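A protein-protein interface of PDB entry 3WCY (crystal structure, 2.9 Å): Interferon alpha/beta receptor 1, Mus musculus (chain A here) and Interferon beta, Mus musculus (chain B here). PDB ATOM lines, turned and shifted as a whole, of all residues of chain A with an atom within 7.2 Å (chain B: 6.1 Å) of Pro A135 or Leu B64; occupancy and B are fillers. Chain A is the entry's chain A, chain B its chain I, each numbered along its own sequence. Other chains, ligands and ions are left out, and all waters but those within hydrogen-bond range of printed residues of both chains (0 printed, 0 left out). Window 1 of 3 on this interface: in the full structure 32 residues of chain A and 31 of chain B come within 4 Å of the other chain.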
ATOM      1  N   TRP A 130     -16.374   8.822  10.117  1.00  0.00           N
ATOM      2  CA  TRP A 130     -17.697   9.362  10.428  1.00  0.00           C
ATOM      3  C   TRP A 130     -17.804  10.045  11.800  1.00  0.00           C
ATOM      4  O   TRP A 130     -18.859  10.593  12.135  1.00  0.00           O
ATOM      5  CB  TRP A 130     -18.773   8.290  10.204  1.00  0.00           C
ATOM      6  CG  TRP A 130     -18.595   7.560   8.905  1.00  0.00           C
ATOM      7  CD1 TRP A 130     -18.134   6.288   8.741  1.00  0.00           C
ATOM      8  CD2 TRP A 130     -18.735   8.110   7.586  1.00  0.00           C
ATOM      9  NE1 TRP A 130     -18.045   5.986   7.401  1.00  0.00           N
ATOM     10  CE2 TRP A 130     -18.395   7.090   6.670  1.00  0.00           C
ATOM     11  CE3 TRP A 130     -19.138   9.362   7.086  1.00  0.00           C
ATOM     12  CZ2 TRP A 130     -18.442   7.281   5.286  1.00  0.00           C
ATOM     13  CZ3 TRP A 130     -19.192   9.546   5.714  1.00  0.00           C
ATOM     14  CH2 TRP A 130     -18.853   8.512   4.830  1.00  0.00           C
ATOM     15  N   ALA A 131     -16.680  10.080  12.550  1.00  0.00           N
ATOM     16  CA  ALA A 131     -16.525  10.692  13.871  1.00  0.00           C
ATOM     17  C   ALA A 131     -17.029  12.139  13.950  1.00  0.00           C
ATOM     18  O   ALA A 131     -17.309  12.620  15.052  1.00  0.00           O
ATOM     19  CB  ALA A 131     -15.069  10.627  14.297  1.00  0.00           C
ATOM     20  N   LEU A 132     -17.137  12.831  12.792  1.00  0.00           N
ATOM     21  CA  LEU A 132     -17.634  14.201  12.693  1.00  0.00           C
ATOM     22  C   LEU A 132     -18.874  14.307  11.807  1.00  0.00           C
ATOM     23  O   LEU A 132     -19.389  15.410  11.616  1.00  0.00           O
ATOM     24  CB  LEU A 132     -16.541  15.151  12.197  1.00  0.00           C
ATOM     25  CG  LEU A 132     -15.263  15.244  13.023  1.00  0.00           C
ATOM     26  CD1 LEU A 132     -14.252  16.162  12.339  1.00  0.00           C
ATOM     27  CD2 LEU A 132     -15.549  15.691  14.466  1.00  0.00           C
ATOM     28  N   GLU A 133     -19.362  13.166  11.276  1.00  0.00           N
ATOM     29  CA  GLU A 133     -20.558  13.117  10.429  1.00  0.00           C
ATOM     30  C   GLU A 133     -21.789  12.564  11.142  1.00  0.00           C
ATOM     31  O   GLU A 133     -22.907  12.784  10.671  1.00  0.00           O
ATOM     32  CB  GLU A 133     -20.287  12.385   9.113  1.00  0.00           C
ATOM     33  CG  GLU A 133     -19.744  13.290   8.022  1.00  0.00           C
ATOM     34  CD  GLU A 133     -18.352  13.840   8.257  1.00  0.00           C
ATOM     35  OE1 GLU A 133     -18.109  15.006   7.869  1.00  0.00           O
ATOM     36  OE2 GLU A 133     -17.506  13.116   8.832  1.00  0.00           O
ATOM     37  N   LYS A 134     -21.589  11.910  12.311  1.00  0.00           N
ATOM     38  CA  LYS A 134     -22.648  11.348  13.164  1.00  0.00           C
ATOM     39  C   LYS A 134     -23.935  12.205  13.240  1.00  0.00           C
ATOM     40  O   LYS A 134     -25.014  11.619  13.095  1.00  0.00           O
ATOM     41  CB  LYS A 134     -22.140  11.067  14.591  1.00  0.00           C
ATOM     42  CG  LYS A 134     -21.012  10.062  14.693  1.00  0.00           C
ATOM     43  CD  LYS A 134     -19.919  10.583  15.609  1.00  0.00           C
ATOM     44  CE  LYS A 134     -20.004  10.028  17.008  1.00  0.00           C
ATOM     45  NZ  LYS A 134     -18.932  10.582  17.868  1.00  0.00           N
ATOM     46  N   PRO A 135     -23.889  13.560  13.461  1.00  0.00           N
ATOM     47  CA  PRO A 135     -25.152  14.315  13.553  1.00  0.00           C
ATOM     48  C   PRO A 135     -25.881  14.456  12.221  1.00  0.00           C
ATOM     49  O   PRO A 135     -27.107  14.596  12.203  1.00  0.00           O
ATOM     50  CB  PRO A 135     -24.718  15.671  14.114  1.00  0.00           C
ATOM     51  CG  PRO A 135     -23.293  15.491  14.572  1.00  0.00           C
ATOM     52  CD  PRO A 135     -22.734  14.459  13.681  1.00  0.00           C
ATOM     53  N   SER A 136     -25.131  14.390  11.109  1.00  0.00           N
ATOM     54  CA  SER A 136     -25.693  14.512   9.767  1.00  0.00           C
ATOM     55  C   SER A 136     -26.561  13.312   9.395  1.00  0.00           C
ATOM     56  O   SER A 136     -27.629  13.513   8.814  1.00  0.00           O
ATOM     57  CB  SER A 136     -24.594  14.738   8.730  1.00  0.00           C
ATOM     58  OG  SER A 136     -24.047  16.045   8.821  1.00  0.00           O
ATOM     59  N   PHE A 137     -26.129  12.082   9.773  1.00  0.00           N
ATOM     60  CA  PHE A 137     -26.826  10.821   9.496  1.00  0.00           C
ATOM     61  C   PHE A 137     -28.285  10.776   9.932  1.00  0.00           C
ATOM     62  O   PHE A 137     -28.646  11.253  11.006  1.00  0.00           O
ATOM     63  CB  PHE A 137     -26.103   9.616  10.123  1.00  0.00           C
ATOM     64  CG  PHE A 137     -24.690   9.313   9.683  1.00  0.00           C
ATOM     65  CD1 PHE A 137     -24.341   9.335   8.338  1.00  0.00           C
ATOM     66  CD2 PHE A 137     -23.737   8.897  10.602  1.00  0.00           C
ATOM     67  CE1 PHE A 137     -23.039   9.029   7.933  1.00  0.00           C
ATOM     68  CE2 PHE A 137     -22.444   8.569  10.192  1.00  0.00           C
ATOM     69  CZ  PHE A 137     -22.106   8.634   8.859  1.00  0.00           C
ATOM     70  N   SER A 138     -29.108  10.164   9.088  1.00  0.00           N
ATOM     71  CA  SER A 138     -30.527   9.905   9.309  1.00  0.00           C
ATOM     72  C   SER A 138     -30.694   8.413   9.061  1.00  0.00           C
ATOM     73  O   SER A 138     -29.800   7.795   8.478  1.00  0.00           O
ATOM     74  CB  SER A 138     -31.386  10.705   8.332  1.00  0.00           C
ATOM     75  OG  SER A 138     -32.767  10.424   8.502  1.00  0.00           O
ATOM     76  N   THR A 157     -34.075   9.986  13.197  1.00  0.00           N
ATOM     77  CA  THR A 157     -32.817  10.683  13.461  1.00  0.00           C
ATOM     78  C   THR A 157     -32.306  10.176  14.810  1.00  0.00           C
ATOM     79  O   THR A 157     -31.115  10.280  15.119  1.00  0.00           O
ATOM     80  CB  THR A 157     -33.049  12.197  13.498  1.00  0.00           C
ATOM     81  OG1 THR A 157     -34.264  12.474  14.206  1.00  0.00           O
ATOM     82  CG2 THR A 157     -33.097  12.813  12.106  1.00  0.00           C
ATOM     83  N   TYR A 159     -31.327   7.533  17.764  1.00  0.00           N
ATOM     84  CA  TYR A 159     -30.505   6.321  17.850  1.00  0.00           C
ATOM     85  C   TYR A 159     -31.215   5.132  18.501  1.00  0.00           C
ATOM     86  O   TYR A 159     -30.675   4.023  18.543  1.00  0.00           O
ATOM     87  CB  TYR A 159     -29.118   6.622  18.441  1.00  0.00           C
ATOM     88  CG  TYR A 159     -28.240   7.388  17.475  1.00  0.00           C
ATOM     89  CD1 TYR A 159     -27.364   6.725  16.622  1.00  0.00           C
ATOM     90  CD2 TYR A 159     -28.322   8.774  17.376  1.00  0.00           C
ATOM     91  CE1 TYR A 159     -26.569   7.426  15.715  1.00  0.00           C
ATOM     92  CE2 TYR A 159     -27.531   9.484  16.473  1.00  0.00           C
ATOM     93  CZ  TYR A 159     -26.653   8.808  15.647  1.00  0.00           C
ATOM     94  OH  TYR A 159     -25.878   9.517  14.761  1.00  0.00           O
ATOM     95  N   HIS A 180     -26.885   9.746   4.574  1.00  0.00           N
ATOM     96  CA  HIS A 180     -26.205  11.042   4.731  1.00  0.00           C
ATOM     97  C   HIS A 180     -27.014  12.017   3.837  1.00  0.00           C
ATOM     98  O   HIS A 180     -26.727  12.117   2.638  1.00  0.00           O
ATOM     99  CB  HIS A 180     -24.723  10.963   4.283  1.00  0.00           C
ATOM    100  CG  HIS A 180     -23.830  12.039   4.843  1.00  0.00           C
ATOM    101  ND1 HIS A 180     -24.311  13.310   5.156  1.00  0.00           N
ATOM    102  CD2 HIS A 180     -22.503  12.004   5.107  1.00  0.00           C
ATOM    103  CE1 HIS A 180     -23.269  13.990   5.608  1.00  0.00           C
ATOM    104  NE2 HIS A 180     -22.159  13.251   5.598  1.00  0.00           N
ATOM    105  N   PRO A 181     -28.076  12.678   4.370  1.00  0.00           N
ATOM    106  CA  PRO A 181     -28.930  13.517   3.509  1.00  0.00           C
ATOM    107  C   PRO A 181     -28.302  14.747   2.862  1.00  0.00           C
ATOM    108  O   PRO A 181     -28.927  15.333   1.974  1.00  0.00           O
ATOM    109  CB  PRO A 181     -30.110  13.880   4.420  1.00  0.00           C
ATOM    110  CG  PRO A 181     -29.575  13.772   5.794  1.00  0.00           C
ATOM    111  CD  PRO A 181     -28.598  12.638   5.753  1.00  0.00           C
ATOM    112  N   SER A 243     -31.289  12.108  20.184  1.00  0.00           N
ATOM    113  CA  SER A 243     -30.818  12.506  18.862  1.00  0.00           C
ATOM    114  C   SER A 243     -29.330  12.254  18.600  1.00  0.00           C
ATOM    115  O   SER A 243     -28.970  12.031  17.446  1.00  0.00           O
ATOM    116  CB  SER A 243     -31.166  13.965  18.597  1.00  0.00           C
ATOM    117  OG  SER A 243     -32.487  14.296  19.000  1.00  0.00           O
ATOM    118  N   SER A 244     -28.463  12.324  19.635  1.00  0.00           N
ATOM    119  CA  SER A 244     -27.020  12.102  19.465  1.00  0.00           C
ATOM    120  C   SER A 244     -26.539  10.699  19.807  1.00  0.00           C
ATOM    121  O   SER A 244     -27.183  10.007  20.601  1.00  0.00           O
ATOM    122  CB  SER A 244     -26.200  13.060  20.325  1.00  0.00           C
ATOM    123  OG  SER A 244     -26.401  12.815  21.707  1.00  0.00           O
ATOM    124  N   SER A 245     -25.458  10.278  19.155  1.00  0.00           N
ATOM    125  CA  SER A 245     -24.969   8.905  19.221  1.00  0.00           C
ATOM    126  C   SER A 245     -24.973   8.264  20.600  1.00  0.00           C
ATOM    127  O   SER A 245     -24.683   8.921  21.601  1.00  0.00           O
ATOM    128  CB  SER A 245     -23.509   8.838  18.764  1.00  0.00           C
ATOM    129  OG  SER A 245     -23.133   7.507  18.452  1.00  0.00           O
ATOM    130  N   LEU B  59     -21.673  24.745  14.590  1.00  0.00           N
ATOM    131  CA  LEU B  59     -22.514  24.375  15.738  1.00  0.00           C
ATOM    132  C   LEU B  59     -22.585  22.849  15.927  1.00  0.00           C
ATOM    133  O   LEU B  59     -22.760  22.368  17.049  1.00  0.00           O
ATOM    134  CB  LEU B  59     -23.945  24.940  15.593  1.00  0.00           C
ATOM    135  CG  LEU B  59     -24.122  26.465  15.523  1.00  0.00           C
ATOM    136  CD1 LEU B  59     -25.514  26.813  15.075  1.00  0.00           C
ATOM    137  CD2 LEU B  59     -23.824  27.137  16.858  1.00  0.00           C
ATOM    138  N   GLN B  60     -22.468  22.096  14.823  1.00  0.00           N
ATOM    139  CA  GLN B  60     -22.473  20.634  14.817  1.00  0.00           C
ATOM    140  C   GLN B  60     -21.159  20.146  15.406  1.00  0.00           C
ATOM    141  O   GLN B  60     -21.138  19.198  16.184  1.00  0.00           O
ATOM    142  CB  GLN B  60     -22.627  20.118  13.380  1.00  0.00           C
ATOM    143  CG  GLN B  60     -23.761  19.131  13.228  1.00  0.00           C
ATOM    144  CD  GLN B  60     -24.137  18.913  11.789  1.00  0.00           C
ATOM    145  OE1 GLN B  60     -25.193  19.361  11.334  1.00  0.00           O
ATOM    146  NE2 GLN B  60     -23.293  18.207  11.046  1.00  0.00           N
ATOM    147  N   ASN B  61     -20.066  20.814  15.045  1.00  0.00           N
ATOM    148  CA  ASN B  61     -18.730  20.481  15.506  1.00  0.00           C
ATOM    149  C   ASN B  61     -18.475  20.920  16.930  1.00  0.00           C
ATOM    150  O   ASN B  61     -17.867  20.157  17.685  1.00  0.00           O
ATOM    151  CB  ASN B  61     -17.705  21.030  14.564  1.00  0.00           C
ATOM    152  CG  ASN B  61     -17.483  20.137  13.391  1.00  0.00           C
ATOM    153  OD1 ASN B  61     -16.831  19.094  13.499  1.00  0.00           O
ATOM    154  ND2 ASN B  61     -18.026  20.524  12.253  1.00  0.00           N
ATOM    155  N   VAL B  62     -18.961  22.128  17.316  1.00  0.00           N
ATOM    156  CA  VAL B  62     -18.869  22.626  18.692  1.00  0.00           C
ATOM    157  C   VAL B  62     -19.607  21.634  19.618  1.00  0.00           C
ATOM    158  O   VAL B  62     -19.081  21.300  20.681  1.00  0.00           O
ATOM    159  CB  VAL B  62     -19.370  24.082  18.836  1.00  0.00           C
ATOM    160  CG1 VAL B  62     -19.517  24.482  20.304  1.00  0.00           C
ATOM    161  CG2 VAL B  62     -18.426  25.051  18.123  1.00  0.00           C
ATOM    162  N   PHE B  63     -20.778  21.105  19.169  1.00  0.00           N
ATOM    163  CA  PHE B  63     -21.562  20.103  19.889  1.00  0.00           C
ATOM    164  C   PHE B  63     -20.669  18.893  20.145  1.00  0.00           C
ATOM    165  O   PHE B  63     -20.379  18.587  21.300  1.00  0.00           O
ATOM    166  CB  PHE B  63     -22.823  19.698  19.084  1.00  0.00           C
ATOM    167  CG  PHE B  63     -23.680  18.636  19.739  1.00  0.00           C
ATOM    168  CD1 PHE B  63     -24.765  18.987  20.534  1.00  0.00           C
ATOM    169  CD2 PHE B  63     -23.389  17.286  19.577  1.00  0.00           C
ATOM    170  CE1 PHE B  63     -25.531  18.006  21.168  1.00  0.00           C
ATOM    171  CE2 PHE B  63     -24.149  16.308  20.226  1.00  0.00           C
ATOM    172  CZ  PHE B  63     -25.221  16.673  21.003  1.00  0.00           C
ATOM    173  N   LEU B  64     -20.194  18.248  19.058  1.00  0.00           N
ATOM    174  CA  LEU B  64     -19.315  17.070  19.056  1.00  0.00           C
ATOM    175  C   LEU B  64     -18.132  17.219  20.015  1.00  0.00           C
ATOM    176  O   LEU B  64     -17.749  16.241  20.653  1.00  0.00           O
ATOM    177  CB  LEU B  64     -18.808  16.791  17.628  1.00  0.00           C
ATOM    178  CG  LEU B  64     -19.746  16.021  16.700  1.00  0.00           C
ATOM    179  CD1 LEU B  64     -19.471  16.366  15.252  1.00  0.00           C
ATOM    180  CD2 LEU B  64     -19.609  14.524  16.906  1.00  0.00           C
ATOM    181  N   VAL B  65     -17.586  18.446  20.137  1.00  0.00           N
ATOM    182  CA  VAL B  65     -16.467  18.772  21.021  1.00  0.00           C
ATOM    183  C   VAL B  65     -16.847  18.580  22.496  1.00  0.00           C
ATOM    184  O   VAL B  65     -16.189  17.807  23.193  1.00  0.00           O
ATOM    185  CB  VAL B  65     -15.867  20.178  20.729  1.00  0.00           C
ATOM    186  CG1 VAL B  65     -15.037  20.684  21.905  1.00  0.00           C
ATOM    187  CG2 VAL B  65     -15.033  20.170  19.450  1.00  0.00           C
ATOM    188  N   PHE B  66     -17.921  19.250  22.954  1.00  0.00           N
ATOM    189  CA  PHE B  66     -18.373  19.173  24.342  1.00  0.00           C
ATOM    190  C   PHE B  66     -18.874  17.812  24.809  1.00  0.00           C
ATOM    191  O   PHE B  66     -19.045  17.616  26.018  1.00  0.00           O
ATOM    192  CB  PHE B  66     -19.331  20.317  24.695  1.00  0.00           C
ATOM    193  CG  PHE B  66     -18.626  21.645  24.793  1.00  0.00           C
ATOM    194  CD1 PHE B  66     -17.873  21.970  25.918  1.00  0.00           C
ATOM    195  CD2 PHE B  66     -18.693  22.561  23.753  1.00  0.00           C
ATOM    196  CE1 PHE B  66     -17.206  23.191  26.003  1.00  0.00           C
ATOM    197  CE2 PHE B  66     -18.027  23.783  23.838  1.00  0.00           C
ATOM    198  CZ  PHE B  66     -17.290  24.092  24.964  1.00  0.00           C
ATOM    199  N   ARG B  67     -19.051  16.855  23.869  1.00  0.00           N
ATOM    200  CA  ARG B  67     -19.458  15.487  24.184  1.00  0.00           C
ATOM    201  C   ARG B  67     -18.329  14.754  24.904  1.00  0.00           C
ATOM    202  O   ARG B  67     -18.593  13.996  25.834  1.00  0.00           O
ATOM    203  CB  ARG B  67     -19.899  14.737  22.922  1.00  0.00           C
ATOM    204  CG  ARG B  67     -21.315  15.089  22.473  1.00  0.00           C
ATOM    205  CD  ARG B  67     -22.365  14.161  23.061  1.00  0.00           C
ATOM    206  NE  ARG B  67     -22.842  13.192  22.073  1.00  0.00           N
ATOM    207  CZ  ARG B  67     -22.470  11.917  22.021  1.00  0.00           C
ATOM    208  NH1 ARG B  67     -21.616  11.429  22.913  1.00  0.00           N
ATOM    209  NH2 ARG B  67     -22.955  11.117  21.082  1.00  0.00           N
ATOM    210  N   ASN B  68     -17.071  15.045  24.521  1.00  0.00           N
ATOM    211  CA  ASN B  68     -15.827  14.489  25.084  1.00  0.00           C
ATOM    212  C   ASN B  68     -15.703  14.642  26.615  1.00  0.00           C
ATOM    213  O   ASN B  68     -16.354  15.515  27.206  1.00  0.00           O
ATOM    214  CB  ASN B  68     -14.619  15.161  24.416  1.00  0.00           C
ATOM    215  CG  ASN B  68     -14.367  14.731  22.995  1.00  0.00           C
ATOM    216  OD1 ASN B  68     -13.997  13.586  22.730  1.00  0.00           O
ATOM    217  ND2 ASN B  68     -14.487  15.659  22.058  1.00  0.00           N
ATOM    218  N   LEU B  84     -24.931  21.819  25.241  1.00  0.00           N
ATOM    219  CA  LEU B  84     -25.127  20.812  24.191  1.00  0.00           C
ATOM    220  C   LEU B  84     -26.563  20.846  23.694  1.00  0.00           C
ATOM    221  O   LEU B  84     -26.790  20.747  22.494  1.00  0.00           O
ATOM    222  CB  LEU B  84     -24.805  19.385  24.682  1.00  0.00           C
ATOM    223  CG  LEU B  84     -23.347  18.986  24.896  1.00  0.00           C
ATOM    224  CD1 LEU B  84     -23.259  17.731  25.736  1.00  0.00           C
ATOM    225  CD2 LEU B  84     -22.647  18.736  23.580  1.00  0.00           C
ATOM    226  N   THR B  91     -28.899  23.481  15.694  1.00  0.00           N
ATOM    227  CA  THR B  91     -28.421  22.541  14.679  1.00  0.00           C
ATOM    228  C   THR B  91     -29.640  21.939  13.959  1.00  0.00           C
ATOM    229  O   THR B  91     -29.678  21.950  12.727  1.00  0.00           O
ATOM    230  CB  THR B  91     -27.513  21.487  15.340  1.00  0.00           C
ATOM    231  OG1 THR B  91     -26.347  22.139  15.847  1.00  0.00           O
ATOM    232  CG2 THR B  91     -27.095  20.377  14.383  1.00  0.00           C
ATOM    233  N   GLN B 125     -10.401  18.063  17.685  1.00  0.00           N
ATOM    234  CA  GLN B 125     -10.749  16.804  18.347  1.00  0.00           C
ATOM    235  C   GLN B 125      -9.496  15.936  18.560  1.00  0.00           C
ATOM    236  O   GLN B 125      -9.385  15.265  19.592  1.00  0.00           O
ATOM    237  CB  GLN B 125     -11.791  16.033  17.522  1.00  0.00           C
ATOM    238  CG  GLN B 125     -12.994  15.562  18.332  1.00  0.00           C
ATOM    239  CD  GLN B 125     -14.221  16.430  18.146  1.00  0.00           C
ATOM    240  OE1 GLN B 125     -14.308  17.277  17.246  1.00  0.00           O
ATOM    241  NE2 GLN B 125     -15.211  16.226  18.991  1.00  0.00           N
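The backbone carbonyl oxygen (O) of Leu B64 lies within hydrogen-bond range of the side-chain amide nitrogen (NE2) of Gln B125 (3.0 Å).
N of Val B65 lies close to NE2 of Gln B125 (3.4 Å).
NE2 of Gln B125 sits close to ND2 of Asn B68.
The side-chain hydroxyl (OG) of Ser A136 sits at hydrogen-bond distance from the side-chain amide nitrogen (NE2) of Gln B60, 3.2 Å away.
The guanidinium group (NH2) of Arg B67 is in hydrogen-bond range of the backbone carbonyl oxygen (O) of Ser A245 (2.8 Å).
Among the printed residues, pairs that only touch across the chains: Ala A131 with Leu B64, Leu A132 with Asn B61, Leu A132 with Leu B64, Leu A132 with Gln B125, Pro A135 with Gln B60, Pro A135 with Leu B64, Ser A244 with Phe B63 and Ser A244 with Arg B67.
Printed residues of chain B within 4 Å of Leu A132: Asn B61 (3.8 Å), Leu B64 (3.8 Å) and Gln B125 (3.4 Å).
Of chain B, only Gln B60 (3.7 Å) and Leu B64 (3.98 Å) come within 4 Å of Pro A135.
Of the printed residues of chain B, Ser A136 touches Gln B60.
Ser A243 touches none of the printed residues of chain B.
Of the printed residues of chain B, Ser A244 touches Phe B63 (3.8 Å) and Arg B67 (3.6 Å).
Of the printed residues of chain A, Gln B60 touches Pro A135 (3.7 Å) and Ser A136 (3.2 Å).
Of chain A, only Ala A131 (3.5 Å), Leu A132 (3.8 Å) and Pro A135 (3.98 Å) come within 4 Å of Leu B64.
The nearest residue of chain A that does not touch Leu B64 is Lys A134 (4.1 Å).
The nearest printed residue of chain B that does not touch Ser A244 is Leu B84 (7.1 Å).
Printed residues of chain B that touch a printed residue of chain A: Gln B60, Asn B61, Phe B63, Leu B64, Arg B67 and Gln B125.
Hydrophobic or aromatic side chains of chain B that line the printed part of chain A: Phe B63 and Leu B64.
Of the 16 printed residues of chain A, 6 touch a printed residue of chain B.
Among the printed residues, 10 pairs touch across the chains.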
